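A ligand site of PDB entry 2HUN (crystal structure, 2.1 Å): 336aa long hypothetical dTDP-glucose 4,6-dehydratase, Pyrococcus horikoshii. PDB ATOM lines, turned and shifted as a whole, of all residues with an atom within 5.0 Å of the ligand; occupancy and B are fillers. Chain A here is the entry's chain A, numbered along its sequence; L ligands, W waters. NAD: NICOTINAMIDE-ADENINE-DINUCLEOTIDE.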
ATOM      1  N   GLY A  10      20.461 -24.225 -10.913  1.00  0.00           N
ATOM      2  CA  GLY A  10      20.017 -25.433 -11.599  1.00  0.00           C
ATOM      3  C   GLY A  10      20.712 -26.664 -11.049  1.00  0.00           C
ATOM      4  O   GLY A  10      20.883 -27.660 -11.743  1.00  0.00           O
ATOM      5  N   MET A  12      19.653 -28.900  -9.007  1.00  0.00           N
ATOM      6  CA  MET A  12      18.820 -30.086  -8.813  1.00  0.00           C
ATOM      7  C   MET A  12      18.627 -30.853 -10.127  1.00  0.00           C
ATOM      8  O   MET A  12      17.862 -31.814 -10.186  1.00  0.00           O
ATOM      9  CB  MET A  12      17.449 -29.701  -8.243  1.00  0.00           C
ATOM     10  CG  MET A  12      16.882 -30.754  -7.307  1.00  0.00           C
ATOM     11  SD  MET A  12      17.892 -30.907  -5.803  1.00  0.00           S
ATOM     12  CE  MET A  12      17.040 -29.685  -4.744  1.00  0.00           C
ATOM     13  N   GLY A  13      19.329 -30.401 -11.167  1.00  0.00           N
ATOM     14  CA  GLY A  13      19.236 -31.051 -12.466  1.00  0.00           C
ATOM     15  C   GLY A  13      20.326 -32.087 -12.701  1.00  0.00           C
ATOM     16  O   GLY A  13      21.125 -32.381 -11.816  1.00  0.00           O
ATOM     17  N   PHE A  14      20.360 -32.625 -13.912  1.00  0.00           N
ATOM     18  CA  PHE A  14      21.332 -33.655 -14.292  1.00  0.00           C
ATOM     19  C   PHE A  14      22.787 -33.281 -14.054  1.00  0.00           C
ATOM     20  O   PHE A  14      23.460 -33.861 -13.201  1.00  0.00           O
ATOM     21  CB  PHE A  14      21.093 -34.027 -15.764  1.00  0.00           C
ATOM     22  CG  PHE A  14      22.179 -34.886 -16.384  1.00  0.00           C
ATOM     23  CD1 PHE A  14      22.816 -35.876 -15.653  1.00  0.00           C
ATOM     24  CD2 PHE A  14      22.508 -34.731 -17.726  1.00  0.00           C
ATOM     25  CE1 PHE A  14      23.774 -36.707 -16.258  1.00  0.00           C
ATOM     26  CE2 PHE A  14      23.465 -35.555 -18.338  1.00  0.00           C
ATOM     27  CZ  PHE A  14      24.095 -36.549 -17.594  1.00  0.00           C
ATOM     28  N   ILE A  15      23.281 -32.301 -14.799  1.00  0.00           N
ATOM     29  CA  ILE A  15      24.668 -31.887 -14.667  1.00  0.00           C
ATOM     30  C   ILE A  15      24.931 -31.139 -13.367  1.00  0.00           C
ATOM     31  O   ILE A  15      25.983 -31.309 -12.746  1.00  0.00           O
ATOM     32  CB  ILE A  15      25.095 -30.999 -15.864  1.00  0.00           C
ATOM     33  CG1 ILE A  15      24.867 -31.775 -17.168  1.00  0.00           C
ATOM     34  CG2 ILE A  15      26.554 -30.589 -15.732  1.00  0.00           C
ATOM     35  CD1 ILE A  15      25.100 -30.954 -18.431  1.00  0.00           C
ATOM     36  N   GLY A  16      23.974 -30.321 -12.942  1.00  0.00           N
ATOM     37  CA  GLY A  16      24.131 -29.574 -11.697  1.00  0.00           C
ATOM     38  C   GLY A  16      24.379 -30.493 -10.512  1.00  0.00           C
ATOM     39  O   GLY A  16      25.285 -30.254  -9.716  1.00  0.00           O
ATOM     40  N   ILE A  35      20.468 -23.116  -5.933  1.00  0.00           N
ATOM     41  CA  ILE A  35      19.209 -22.436  -6.180  1.00  0.00           C
ATOM     42  C   ILE A  35      18.606 -23.106  -7.399  1.00  0.00           C
ATOM     43  O   ILE A  35      19.222 -23.159  -8.465  1.00  0.00           O
ATOM     44  CB  ILE A  35      19.405 -20.907  -6.417  1.00  0.00           C
ATOM     45  CG1 ILE A  35      18.053 -20.262  -6.711  1.00  0.00           C
ATOM     46  CG2 ILE A  35      20.394 -20.666  -7.545  1.00  0.00           C
ATOM     47  CD1 ILE A  35      18.096 -18.753  -6.808  1.00  0.00           C
ATOM     48  N   ASP A  36      17.421 -23.667  -7.214  1.00  0.00           N
ATOM     49  CA  ASP A  36      16.731 -24.364  -8.281  1.00  0.00           C
ATOM     50  C   ASP A  36      15.268 -24.119  -8.039  1.00  0.00           C
ATOM     51  O   ASP A  36      14.777 -24.134  -6.917  1.00  0.00           O
ATOM     52  CB  ASP A  36      17.040 -25.865  -8.226  1.00  0.00           C
ATOM     53  CG  ASP A  36      16.763 -26.564  -9.547  1.00  0.00           C
ATOM     54  OD1 ASP A  36      15.588 -26.672  -9.944  1.00  0.00           O
ATOM     55  OD2 ASP A  36      17.733 -27.025 -10.190  1.00  0.00           O
ATOM     56  N   LYS A  37      14.587 -23.918  -9.141  1.00  0.00           N
ATOM     57  CA  LYS A  37      13.187 -23.615  -9.158  1.00  0.00           C
ATOM     58  C   LYS A  37      12.307 -24.876  -9.071  1.00  0.00           C
ATOM     59  O   LYS A  37      11.091 -24.801  -8.845  1.00  0.00           O
ATOM     60  CB  LYS A  37      12.984 -22.810 -10.432  1.00  0.00           C
ATOM     61  CG  LYS A  37      13.030 -23.585 -11.757  1.00  0.00           C
ATOM     62  CD  LYS A  37      12.570 -22.687 -12.948  1.00  0.00           C
ATOM     63  CE  LYS A  37      12.157 -23.534 -14.169  1.00  0.00           C
ATOM     64  NZ  LYS A  37      11.770 -22.717 -15.363  1.00  0.00           N
ATOM     65  N   LEU A  38      12.942 -26.031  -9.245  1.00  0.00           N
ATOM     66  CA  LEU A  38      12.288 -27.333  -9.228  1.00  0.00           C
ATOM     67  C   LEU A  38      11.273 -27.460 -10.346  1.00  0.00           C
ATOM     68  O   LEU A  38      10.113 -27.809 -10.115  1.00  0.00           O
ATOM     69  CB  LEU A  38      11.619 -27.596  -7.873  1.00  0.00           C
ATOM     70  CG  LEU A  38      12.544 -27.662  -6.650  1.00  0.00           C
ATOM     71  CD1 LEU A  38      11.749 -28.153  -5.439  1.00  0.00           C
ATOM     72  CD2 LEU A  38      13.727 -28.609  -6.924  1.00  0.00           C
ATOM     73  N   GLY A  39      11.706 -27.156 -11.560  1.00  0.00           N
ATOM     74  CA  GLY A  39      10.826 -27.271 -12.712  1.00  0.00           C
ATOM     75  C   GLY A  39      11.251 -28.435 -13.587  1.00  0.00           C
ATOM     76  O   GLY A  39      11.795 -29.422 -13.104  1.00  0.00           O
ATOM     77  N   TYR A  40      10.976 -28.330 -14.879  1.00  0.00           N
ATOM     78  CA  TYR A  40      11.332 -29.382 -15.832  1.00  0.00           C
ATOM     79  C   TYR A  40      12.786 -29.851 -15.675  1.00  0.00           C
ATOM     80  O   TYR A  40      13.725 -29.038 -15.711  1.00  0.00           O
ATOM     81  CB  TYR A  40      11.111 -28.878 -17.263  1.00  0.00           C
ATOM     82  CG  TYR A  40      11.560 -29.866 -18.322  1.00  0.00           C
ATOM     83  CD1 TYR A  40      10.767 -30.971 -18.639  1.00  0.00           C
ATOM     84  CD2 TYR A  40      12.803 -29.739 -18.942  1.00  0.00           C
ATOM     85  CE1 TYR A  40      11.212 -31.929 -19.557  1.00  0.00           C
ATOM     86  CE2 TYR A  40      13.247 -30.686 -19.849  1.00  0.00           C
ATOM     87  CZ  TYR A  40      12.456 -31.768 -20.159  1.00  0.00           C
ATOM     88  OH  TYR A  40      12.911 -32.703 -21.056  1.00  0.00           O
ATOM     89  N   GLY A  41      12.961 -31.153 -15.495  1.00  0.00           N
ATOM     90  CA  GLY A  41      14.295 -31.711 -15.365  1.00  0.00           C
ATOM     91  C   GLY A  41      14.819 -31.858 -13.954  1.00  0.00           C
ATOM     92  O   GLY A  41      15.744 -32.636 -13.713  1.00  0.00           O
ATOM     93  N   SER A  42      14.241 -31.128 -12.999  1.00  0.00           N
ATOM     94  CA  SER A  42      14.702 -31.204 -11.623  1.00  0.00           C
ATOM     95  C   SER A  42      14.283 -32.504 -10.943  1.00  0.00           C
ATOM     96  O   SER A  42      13.257 -33.089 -11.261  1.00  0.00           O
ATOM     97  CB  SER A  42      14.153 -30.019 -10.808  1.00  0.00           C
ATOM     98  OG  SER A  42      12.743 -30.078 -10.683  1.00  0.00           O
ATOM     99  N   GLY A  61      13.940 -21.362  -5.759  1.00  0.00           N
ATOM    100  CA  GLY A  61      13.652 -20.067  -6.346  1.00  0.00           C
ATOM    101  C   GLY A  61      14.096 -19.970  -7.786  1.00  0.00           C
ATOM    102  O   GLY A  61      14.806 -20.839  -8.295  1.00  0.00           O
ATOM    103  N   ASP A  62      13.684 -18.890  -8.436  1.00  0.00           N
ATOM    104  CA  ASP A  62      13.987 -18.623  -9.846  1.00  0.00           C
ATOM    105  C   ASP A  62      15.155 -17.632  -9.953  1.00  0.00           C
ATOM    106  O   ASP A  62      15.119 -16.575  -9.331  1.00  0.00           O
ATOM    107  CB  ASP A  62      12.734 -18.017 -10.497  1.00  0.00           C
ATOM    108  CG  ASP A  62      12.882 -17.826 -11.987  1.00  0.00           C
ATOM    109  OD1 ASP A  62      14.020 -17.778 -12.487  1.00  0.00           O
ATOM    110  OD2 ASP A  62      11.843 -17.675 -12.657  1.00  0.00           O
ATOM    111  N   VAL A  63      16.163 -17.955 -10.747  1.00  0.00           N
ATOM    112  CA  VAL A  63      17.299 -17.054 -10.921  1.00  0.00           C
ATOM    113  C   VAL A  63      16.840 -15.701 -11.442  1.00  0.00           C
ATOM    114  O   VAL A  63      17.568 -14.708 -11.362  1.00  0.00           O
ATOM    115  CB  VAL A  63      18.359 -17.625 -11.902  1.00  0.00           C
ATOM    116  CG1 VAL A  63      19.071 -18.804 -11.278  1.00  0.00           C
ATOM    117  CG2 VAL A  63      17.702 -18.023 -13.217  1.00  0.00           C
ATOM    118  N   ALA A  64      15.622 -15.663 -11.987  1.00  0.00           N
ATOM    119  CA  ALA A  64      15.055 -14.430 -12.511  1.00  0.00           C
ATOM    120  C   ALA A  64      14.437 -13.589 -11.390  1.00  0.00           C
ATOM    121  O   ALA A  64      13.889 -12.512 -11.648  1.00  0.00           O
ATOM    122  CB  ALA A  64      13.988 -14.762 -13.553  1.00  0.00           C
ATOM    123  N   HIS A  81      26.572 -21.204 -13.214  1.00  0.00           N
ATOM    124  CA  HIS A  81      25.232 -21.038 -13.813  1.00  0.00           C
ATOM    125  C   HIS A  81      24.766 -22.205 -14.720  1.00  0.00           C
ATOM    126  O   HIS A  81      25.008 -22.231 -15.917  1.00  0.00           O
ATOM    127  CB  HIS A  81      25.229 -19.728 -14.606  1.00  0.00           C
ATOM    128  CG  HIS A  81      23.811 -19.375 -14.975  1.00  0.00           C
ATOM    129  ND1 HIS A  81      22.756 -19.514 -14.129  1.00  0.00           N
ATOM    130  CD2 HIS A  81      23.339 -18.840 -16.177  1.00  0.00           C
ATOM    131  CE1 HIS A  81      21.679 -19.077 -14.813  1.00  0.00           C
ATOM    132  NE2 HIS A  81      22.000 -18.667 -16.048  1.00  0.00           N
ATOM    133  N   LEU A  82      24.050 -23.189 -14.184  1.00  0.00           N
ATOM    134  CA  LEU A  82      23.547 -24.288 -14.994  1.00  0.00           C
ATOM    135  C   LEU A  82      22.049 -24.189 -15.275  1.00  0.00           C
ATOM    136  O   LEU A  82      21.545 -24.826 -16.199  1.00  0.00           O
ATOM    137  CB  LEU A  82      23.838 -25.622 -14.306  1.00  0.00           C
ATOM    138  CG  LEU A  82      25.328 -25.955 -14.218  1.00  0.00           C
ATOM    139  CD1 LEU A  82      25.684 -26.406 -12.811  1.00  0.00           C
ATOM    140  CD2 LEU A  82      25.667 -27.018 -15.236  1.00  0.00           C
ATOM    141  N   ALA A  83      21.341 -23.378 -14.502  1.00  0.00           N
ATOM    142  CA  ALA A  83      19.906 -23.207 -14.668  1.00  0.00           C
ATOM    143  C   ALA A  83      19.465 -22.768 -16.061  1.00  0.00           C
ATOM    144  O   ALA A  83      19.938 -21.753 -16.591  1.00  0.00           O
ATOM    145  CB  ALA A  83      19.366 -22.233 -13.625  1.00  0.00           C
ATOM    146  N   ALA A  84      18.528 -23.510 -16.638  1.00  0.00           N
ATOM    147  CA  ALA A  84      18.010 -23.207 -17.970  1.00  0.00           C
ATOM    148  C   ALA A  84      16.889 -24.162 -18.350  1.00  0.00           C
ATOM    149  O   ALA A  84      16.770 -25.238 -17.761  1.00  0.00           O
ATOM    150  CB  ALA A  84      19.129 -23.305 -19.010  1.00  0.00           C
ATOM    151  N   GLU A  85      16.088 -23.760 -19.326  1.00  0.00           N
ATOM    152  CA  GLU A  85      15.006 -24.581 -19.874  1.00  0.00           C
ATOM    153  C   GLU A  85      15.667 -25.110 -21.149  1.00  0.00           C
ATOM    154  O   GLU A  85      16.155 -24.315 -21.973  1.00  0.00           O
ATOM    155  CB  GLU A  85      13.803 -23.712 -20.240  1.00  0.00           C
ATOM    156  CG  GLU A  85      12.916 -23.305 -19.064  1.00  0.00           C
ATOM    157  CD  GLU A  85      12.127 -24.486 -18.497  1.00  0.00           C
ATOM    158  OE1 GLU A  85      11.895 -25.468 -19.233  1.00  0.00           O
ATOM    159  OE2 GLU A  85      11.720 -24.416 -17.320  1.00  0.00           O
ATOM    160  N   SER A  86      15.699 -26.431 -21.329  1.00  0.00           N
ATOM    161  CA  SER A  86      16.404 -26.989 -22.484  1.00  0.00           C
ATOM    162  C   SER A  86      15.696 -27.975 -23.394  1.00  0.00           C
ATOM    163  O   SER A  86      16.332 -28.662 -24.177  1.00  0.00           O
ATOM    164  CB  SER A  86      17.695 -27.651 -22.003  1.00  0.00           C
ATOM    165  OG  SER A  86      17.389 -28.707 -21.107  1.00  0.00           O
ATOM    166  N   HIS A 100      12.420 -16.350 -20.702  1.00  0.00           N
ATOM    167  CA  HIS A 100      12.427 -16.038 -19.282  1.00  0.00           C
ATOM    168  C   HIS A 100      13.562 -16.660 -18.477  1.00  0.00           C
ATOM    169  O   HIS A 100      14.319 -15.973 -17.803  1.00  0.00           O
ATOM    170  CB  HIS A 100      11.114 -16.456 -18.637  1.00  0.00           C
ATOM    171  CG  HIS A 100      11.068 -16.222 -17.160  1.00  0.00           C
ATOM    172  ND1 HIS A 100      10.907 -14.977 -16.604  1.00  0.00           N
ATOM    173  CD2 HIS A 100      11.218 -17.083 -16.127  1.00  0.00           C
ATOM    174  CE1 HIS A 100      10.942 -15.072 -15.284  1.00  0.00           C
ATOM    175  NE2 HIS A 100      11.135 -16.343 -14.968  1.00  0.00           N
ATOM    176  N   SER A 101      13.670 -17.981 -18.528  1.00  0.00           N
ATOM    177  CA  SER A 101      14.713 -18.677 -17.781  1.00  0.00           C
ATOM    178  C   SER A 101      16.120 -18.512 -18.361  1.00  0.00           C
ATOM    179  O   SER A 101      17.074 -18.285 -17.624  1.00  0.00           O
ATOM    180  CB  SER A 101      14.393 -20.177 -17.652  1.00  0.00           C
ATOM    181  OG  SER A 101      13.268 -20.405 -16.812  1.00  0.00           O
ATOM    182  N   VAL A 125      27.307 -21.628 -18.103  1.00  0.00           N
ATOM    183  CA  VAL A 125      27.270 -22.896 -18.833  1.00  0.00           C
ATOM    184  C   VAL A 125      26.326 -22.805 -20.044  1.00  0.00           C
ATOM    185  O   VAL A 125      25.147 -22.440 -19.922  1.00  0.00           O
ATOM    186  CB  VAL A 125      26.818 -24.062 -17.909  1.00  0.00           C
ATOM    187  CG1 VAL A 125      26.872 -25.390 -18.668  1.00  0.00           C
ATOM    188  CG2 VAL A 125      27.721 -24.127 -16.682  1.00  0.00           C
ATOM    189  N   SER A 126      26.847 -23.145 -21.217  1.00  0.00           N
ATOM    190  CA  SER A 126      26.055 -23.059 -22.440  1.00  0.00           C
ATOM    191  C   SER A 126      26.163 -24.349 -23.267  1.00  0.00           C
ATOM    192  O   SER A 126      26.731 -25.341 -22.805  1.00  0.00           O
ATOM    193  CB  SER A 126      26.500 -21.834 -23.251  1.00  0.00           C
ATOM    194  OG  SER A 126      25.582 -21.528 -24.289  1.00  0.00           O
ATOM    195  N   THR A 127      25.645 -24.306 -24.500  1.00  0.00           N
ATOM    196  CA  THR A 127      25.606 -25.494 -25.361  1.00  0.00           C
ATOM    197  C   THR A 127      26.232 -25.418 -26.750  1.00  0.00           C
ATOM    198  O   THR A 127      26.344 -24.343 -27.351  1.00  0.00           O
ATOM    199  CB  THR A 127      24.147 -25.936 -25.552  1.00  0.00           C
ATOM    200  OG1 THR A 127      24.090 -27.008 -26.495  1.00  0.00           O
ATOM    201  CG2 THR A 127      23.314 -24.785 -26.062  1.00  0.00           C
ATOM    202  N   ASP A 128      26.615 -26.587 -27.262  1.00  0.00           N
ATOM    203  CA  ASP A 128      27.210 -26.711 -28.587  1.00  0.00           C
ATOM    204  C   ASP A 128      26.165 -26.370 -29.657  1.00  0.00           C
ATOM    205  O   ASP A 128      26.506 -26.122 -30.814  1.00  0.00           O
ATOM    206  CB  ASP A 128      27.752 -28.133 -28.795  1.00  0.00           C
ATOM    207  CG  ASP A 128      26.648 -29.217 -28.785  1.00  0.00           C
ATOM    208  OD1 ASP A 128      25.579 -29.000 -28.181  1.00  0.00           O
ATOM    209  OD2 ASP A 128      26.865 -30.284 -29.386  1.00  0.00           O
ATOM    210  N   TYR A 151      15.191 -22.522 -28.151  1.00  0.00           N
ATOM    211  CA  TYR A 151      16.034 -22.942 -27.045  1.00  0.00           C
ATOM    212  C   TYR A 151      17.478 -22.496 -27.250  1.00  0.00           C
ATOM    213  O   TYR A 151      18.057 -21.822 -26.398  1.00  0.00           O
ATOM    214  CB  TYR A 151      16.005 -24.466 -26.868  1.00  0.00           C
ATOM    215  CG  TYR A 151      17.200 -25.011 -26.109  1.00  0.00           C
ATOM    216  CD1 TYR A 151      17.419 -24.662 -24.781  1.00  0.00           C
ATOM    217  CD2 TYR A 151      18.131 -25.851 -26.732  1.00  0.00           C
ATOM    218  CE1 TYR A 151      18.535 -25.118 -24.079  1.00  0.00           C
ATOM    219  CE2 TYR A 151      19.250 -26.323 -26.033  1.00  0.00           C
ATOM    220  CZ  TYR A 151      19.451 -25.946 -24.717  1.00  0.00           C
ATOM    221  OH  TYR A 151      20.540 -26.414 -24.009  1.00  0.00           O
ATOM    222  N   LYS A 155      19.739 -19.471 -25.518  1.00  0.00           N
ATOM    223  CA  LYS A 155      21.009 -19.777 -24.862  1.00  0.00           C
ATOM    224  C   LYS A 155      22.056 -18.854 -25.488  1.00  0.00           C
ATOM    225  O   LYS A 155      22.891 -18.285 -24.799  1.00  0.00           O
ATOM    226  CB  LYS A 155      21.414 -21.242 -25.077  1.00  0.00           C
ATOM    227  CG  LYS A 155      20.598 -22.246 -24.268  1.00  0.00           C
ATOM    228  CD  LYS A 155      20.770 -22.064 -22.759  1.00  0.00           C
ATOM    229  CE  LYS A 155      22.189 -22.436 -22.311  1.00  0.00           C
ATOM    230  NZ  LYS A 155      22.404 -22.209 -20.849  1.00  0.00           N
ATOM    231  N   CYS A 178      29.465 -27.140 -24.063  1.00  0.00           N
ATOM    232  CA  CYS A 178      29.758 -28.567 -24.158  1.00  0.00           C
ATOM    233  C   CYS A 178      28.787 -29.335 -25.032  1.00  0.00           C
ATOM    234  O   CYS A 178      27.672 -28.890 -25.314  1.00  0.00           O
ATOM    235  CB  CYS A 178      29.727 -29.181 -22.753  1.00  0.00           C
ATOM    236  SG  CYS A 178      28.072 -29.156 -22.043  1.00  0.00           S
ATOM    237  N   THR A 179      29.213 -30.524 -25.432  1.00  0.00           N
ATOM    238  CA  THR A 179      28.411 -31.403 -26.268  1.00  0.00           C
ATOM    239  C   THR A 179      27.446 -32.195 -25.389  1.00  0.00           C
ATOM    240  O   THR A 179      27.160 -31.798 -24.264  1.00  0.00           O
ATOM    241  CB  THR A 179      29.315 -32.372 -27.051  1.00  0.00           C
ATOM    242  OG1 THR A 179      30.037 -33.197 -26.133  1.00  0.00           O
ATOM    243  CG2 THR A 179      30.304 -31.599 -27.895  1.00  0.00           C
ATOM    244  N   ASN A 180      26.966 -33.325 -25.898  1.00  0.00           N
ATOM    245  CA  ASN A 180      26.010 -34.135 -25.163  1.00  0.00           C
ATOM    246  C   ASN A 180      26.572 -34.852 -23.940  1.00  0.00           C
ATOM    247  O   ASN A 180      27.547 -35.597 -24.048  1.00  0.00           O
ATOM    248  CB  ASN A 180      25.397 -35.163 -26.112  1.00  0.00           C
ATOM    249  CG  ASN A 180      24.815 -34.531 -27.345  1.00  0.00           C
ATOM    250  OD1 ASN A 180      23.783 -33.856 -27.281  1.00  0.00           O
ATOM    251  ND2 ASN A 180      25.480 -34.719 -28.476  1.00  0.00           N
ATOM    252  N   ASN A 181      25.967 -34.605 -22.774  1.00  0.00           N
ATOM    253  CA  ASN A 181      26.394 -35.255 -21.537  1.00  0.00           C
ATOM    254  C   ASN A 181      25.624 -36.551 -21.318  1.00  0.00           C
ATOM    255  O   ASN A 181      24.476 -36.679 -21.739  1.00  0.00           O
ATOM    256  CB  ASN A 181      26.148 -34.347 -20.320  1.00  0.00           C
ATOM    257  CG  ASN A 181      27.196 -33.267 -20.145  1.00  0.00           C
ATOM    258  OD1 ASN A 181      27.673 -33.026 -19.039  1.00  0.00           O
ATOM    259  ND2 ASN A 181      27.543 -32.593 -21.245  1.00  0.00           N
HETATM  260  PA  NAD L   1      18.164 -30.241 -16.625  1.00  0.00           P
HETATM  261  O1A NAD L   1      16.949 -29.968 -17.418  1.00  0.00           O
HETATM  262  O2A NAD L   1      18.414 -31.626 -16.119  1.00  0.00           O
HETATM  263  O5B NAD L   1      18.115 -29.282 -15.345  1.00  0.00           O
HETATM  264  C5B NAD L   1      17.966 -27.860 -15.427  1.00  0.00           C
HETATM  265  C4B NAD L   1      17.851 -27.404 -13.965  1.00  0.00           C
HETATM  266  O4B NAD L   1      17.751 -25.967 -13.888  1.00  0.00           O
HETATM  267  C3B NAD L   1      16.574 -27.985 -13.300  1.00  0.00           C
HETATM  268  O3B NAD L   1      16.883 -28.512 -12.000  1.00  0.00           O
HETATM  269  C2B NAD L   1      15.601 -26.795 -13.309  1.00  0.00           C
HETATM  270  O2B NAD L   1      14.587 -26.795 -12.309  1.00  0.00           O
HETATM  271  C1B NAD L   1      16.567 -25.609 -13.189  1.00  0.00           C
HETATM  272  N9A NAD L   1      16.040 -24.347 -13.774  1.00  0.00           N
HETATM  273  C8A NAD L   1      15.562 -24.128 -15.012  1.00  0.00           C
HETATM  274  N7A NAD L   1      15.195 -22.850 -15.119  1.00  0.00           N
HETATM  275  C5A NAD L   1      15.432 -22.246 -13.966  1.00  0.00           C
HETATM  276  C6A NAD L   1      15.258 -20.922 -13.473  1.00  0.00           C
HETATM  277  N6A NAD L   1      14.744 -19.939 -14.200  1.00  0.00           N
HETATM  278  N1A NAD L   1      15.646 -20.673 -12.138  1.00  0.00           N
HETATM  279  C2A NAD L   1      16.180 -21.699 -11.343  1.00  0.00           C
HETATM  280  N3A NAD L   1      16.353 -22.943 -11.815  1.00  0.00           N
HETATM  281  C4A NAD L   1      15.979 -23.203 -13.094  1.00  0.00           C
HETATM  282  O3  NAD L   1      19.351 -29.963 -17.635  1.00  0.00           O
HETATM  283  PN  NAD L   1      20.924 -30.072 -17.623  1.00  0.00           P
HETATM  284  O1N NAD L   1      21.181 -31.022 -18.744  1.00  0.00           O
HETATM  285  O2N NAD L   1      21.438 -30.504 -16.303  1.00  0.00           O
HETATM  286  O5D NAD L   1      21.447 -28.630 -18.128  1.00  0.00           O
HETATM  287  C5D NAD L   1      22.347 -27.796 -17.388  1.00  0.00           C
HETATM  288  C4D NAD L   1      22.950 -26.738 -18.352  1.00  0.00           C
HETATM  289  O4D NAD L   1      23.880 -27.355 -19.263  1.00  0.00           O
HETATM  290  C3D NAD L   1      21.890 -26.009 -19.177  1.00  0.00           C
HETATM  291  O3D NAD L   1      22.215 -24.601 -19.200  1.00  0.00           O
HETATM  292  C2D NAD L   1      22.017 -26.667 -20.583  1.00  0.00           C
HETATM  293  O2D NAD L   1      21.644 -25.727 -21.593  1.00  0.00           O
HETATM  294  C1D NAD L   1      23.483 -27.046 -20.606  1.00  0.00           C
HETATM  295  N1N NAD L   1      23.818 -28.192 -21.479  1.00  0.00           N
HETATM  296  C2N NAD L   1      23.377 -29.531 -21.194  1.00  0.00           C
HETATM  297  C3N NAD L   1      23.748 -30.562 -22.074  1.00  0.00           C
HETATM  298  C7N NAD L   1      23.318 -32.031 -21.817  1.00  0.00           C
HETATM  299  O7N NAD L   1      23.816 -32.929 -22.518  1.00  0.00           O
HETATM  300  N7N NAD L   1      22.441 -32.302 -20.857  1.00  0.00           N
HETATM  301  C4N NAD L   1      24.545 -30.290 -23.216  1.00  0.00           C
HETATM  302  C5N NAD L   1      24.967 -28.970 -23.475  1.00  0.00           C
HETATM  303  C6N NAD L   1      24.605 -27.909 -22.624  1.00  0.00           C
HETATM  304  O   HOH W   1      17.311 -33.703 -15.250  1.00  0.00           O
HETATM  305  O   HOH W   2      21.443 -29.146 -14.151  1.00  0.00           O
HETATM  306  O   HOH W   3      19.150 -33.288 -19.328  1.00  0.00           O
HETATM  307  O   HOH W   4      15.800 -27.855 -18.661  1.00  0.00           O
HETATM  308  O   HOH W   5      16.610 -32.151 -19.101  1.00  0.00           O
HETATM  309  O   HOH W   6      24.320 -30.917 -26.376  1.00  0.00           O
HETATM  310  O   HOH W   7      22.666 -35.320 -23.955  1.00  0.00           O
HETATM  311  O   HOH W   8      20.755 -34.630 -20.925  1.00  0.00           O
HETATM  312  O   HOH W   9      13.768 -26.059 -16.295  1.00  0.00           O
HETATM  313  O   HOH W  10      19.492 -30.328 -20.929  1.00  0.00           O
HETATM  314  O   HOH W  11      22.583 -22.212 -17.588  1.00  0.00           O
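The side-chain amino group (NZ) of Lys 37 sits close to a nitrogen (N7A) of the ligand (3.4 Å). The side-chain carboxylate (OD1) of Asp 62 lies within hydrogen-bond range of a nitrogen (N6A) of the ligand (2.9 Å). OH of Tyr 151 sits at hydrogen-bond distance from O2D of the ligand (2.7 Å). The backbone carbonyl oxygen (O) of Leu 82 sits at hydrogen-bond distance from an oxygen (O3D) of the ligand (3.1 Å). An oxygen (O2N) of the ligand sits at hydrogen-bond distance from the backbone NH of Ile 15 (3.0 Å). The backbone NH (N) of Asn 181 is in hydrogen-bond range of an oxygen (O7N) of the ligand. A nitrogen (N3A) of the ligand lies within hydrogen-bond range of the backbone NH of Lys 37 (3.3 Å). The side-chain amino group (NZ) of Lys 155 is in hydrogen-bond range of an oxygen (O3D) of the ligand, at 2.9 Å. The side-chain carboxylate (OD2) of Asp 36 lies within hydrogen-bond range of an oxygen (O3B) of the ligand (2.5 Å). N of Gly 39 is in hydrogen-bond range of O2B of the ligand (3.0 Å). OG of Ser 101 lies within hydrogen-bond range of N6A of the ligand (3.0 Å). The backbone NH of Phe 14 lies within hydrogen-bond range of an oxygen (O2A) of the ligand, at 3.1 Å. The backbone NH (N) of Val 63 lies within hydrogen-bond range of a nitrogen (N1A) of the ligand (3.1 Å). An oxygen (O3B) of the ligand lies within hydrogen-bond range of the backbone NH of Gly 13, 3.2 Å away.
The side-chain carboxylate (OE2) of Glu 85 lies within salt-bridge range of the side-chain amino group (NZ) of Lys 37, at 2.6 Å. ND2 of Asn 181 is in hydrogen-bond range of SG of Cys 178 (3.6 Å). N of Ala 64 lies within hydrogen-bond range of OD1 of Asp 62 (2.7 Å). OG of Ser 101 lies within hydrogen-bond range of NZ of Lys 37 (3.1 Å). The side-chain amino group (NZ) of Lys 155 lies within hydrogen-bond range of the backbone carbonyl oxygen (O) of Val 125 (2.9 Å). The side-chain carboxylate (OD2) of Asp 62 is in hydrogen-bond range of a ring nitrogen (NE2) of His 100, at 2.8 Å. The side-chain amide nitrogen (ND2) of Asn 181 lies within hydrogen-bond range of the backbone carbonyl oxygen (O) of Thr 179, 3.1 Å away. OG1 of Thr 127 lies within hydrogen-bond range of OD1 of Asp 128 (3.0 Å).
Merely in contact with the ligand: Gly 10, Met 12, Leu 38, Tyr 40, Gly 41, Ser 42, Gly 61, Ala 83, Ala 84, Ser 86, Val 125, Ser 126, Thr 127, Cys 178, Thr 179 and Asn 180. The nearest printed residue that does not touch the ligand is Gly 16 (4.2 Å).
Water W1 lies within hydrogen-bond range of O of Gly 41 (2.4 Å), O2A of the ligand (2.5 Å) and N of Phe 14 (3.5 Å). Water W2 lies within hydrogen-bond range of an oxygen (O2N) of the ligand (2.5 Å), the backbone carbonyl oxygen (O) of Gly 10 (2.9 Å) and the backbone NH (N) of Gly 16 (3.0 Å). Water W4 lies within hydrogen-bond range of an oxygen (O1A) of the ligand (2.7 Å), the backbone carbonyl oxygen (O) of Ala 84 (2.9 Å) and the backbone NH (N) of Ser 86 (3.0 Å). Water W10 lies within hydrogen-bond range of the side-chain hydroxyl of Ser 86 and an oxygen (O1N) of the ligand. Water W7 lies within hydrogen-bond range of an oxygen (O7N) of the ligand (3.0 Å) and the backbone carbonyl oxygen of Asn 181 (3.2 Å). Water W6 lies within hydrogen-bond range of the side-chain carboxylate (OD1) of Asp 128 and the side-chain amide oxygen (OD1) of Asn 180.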
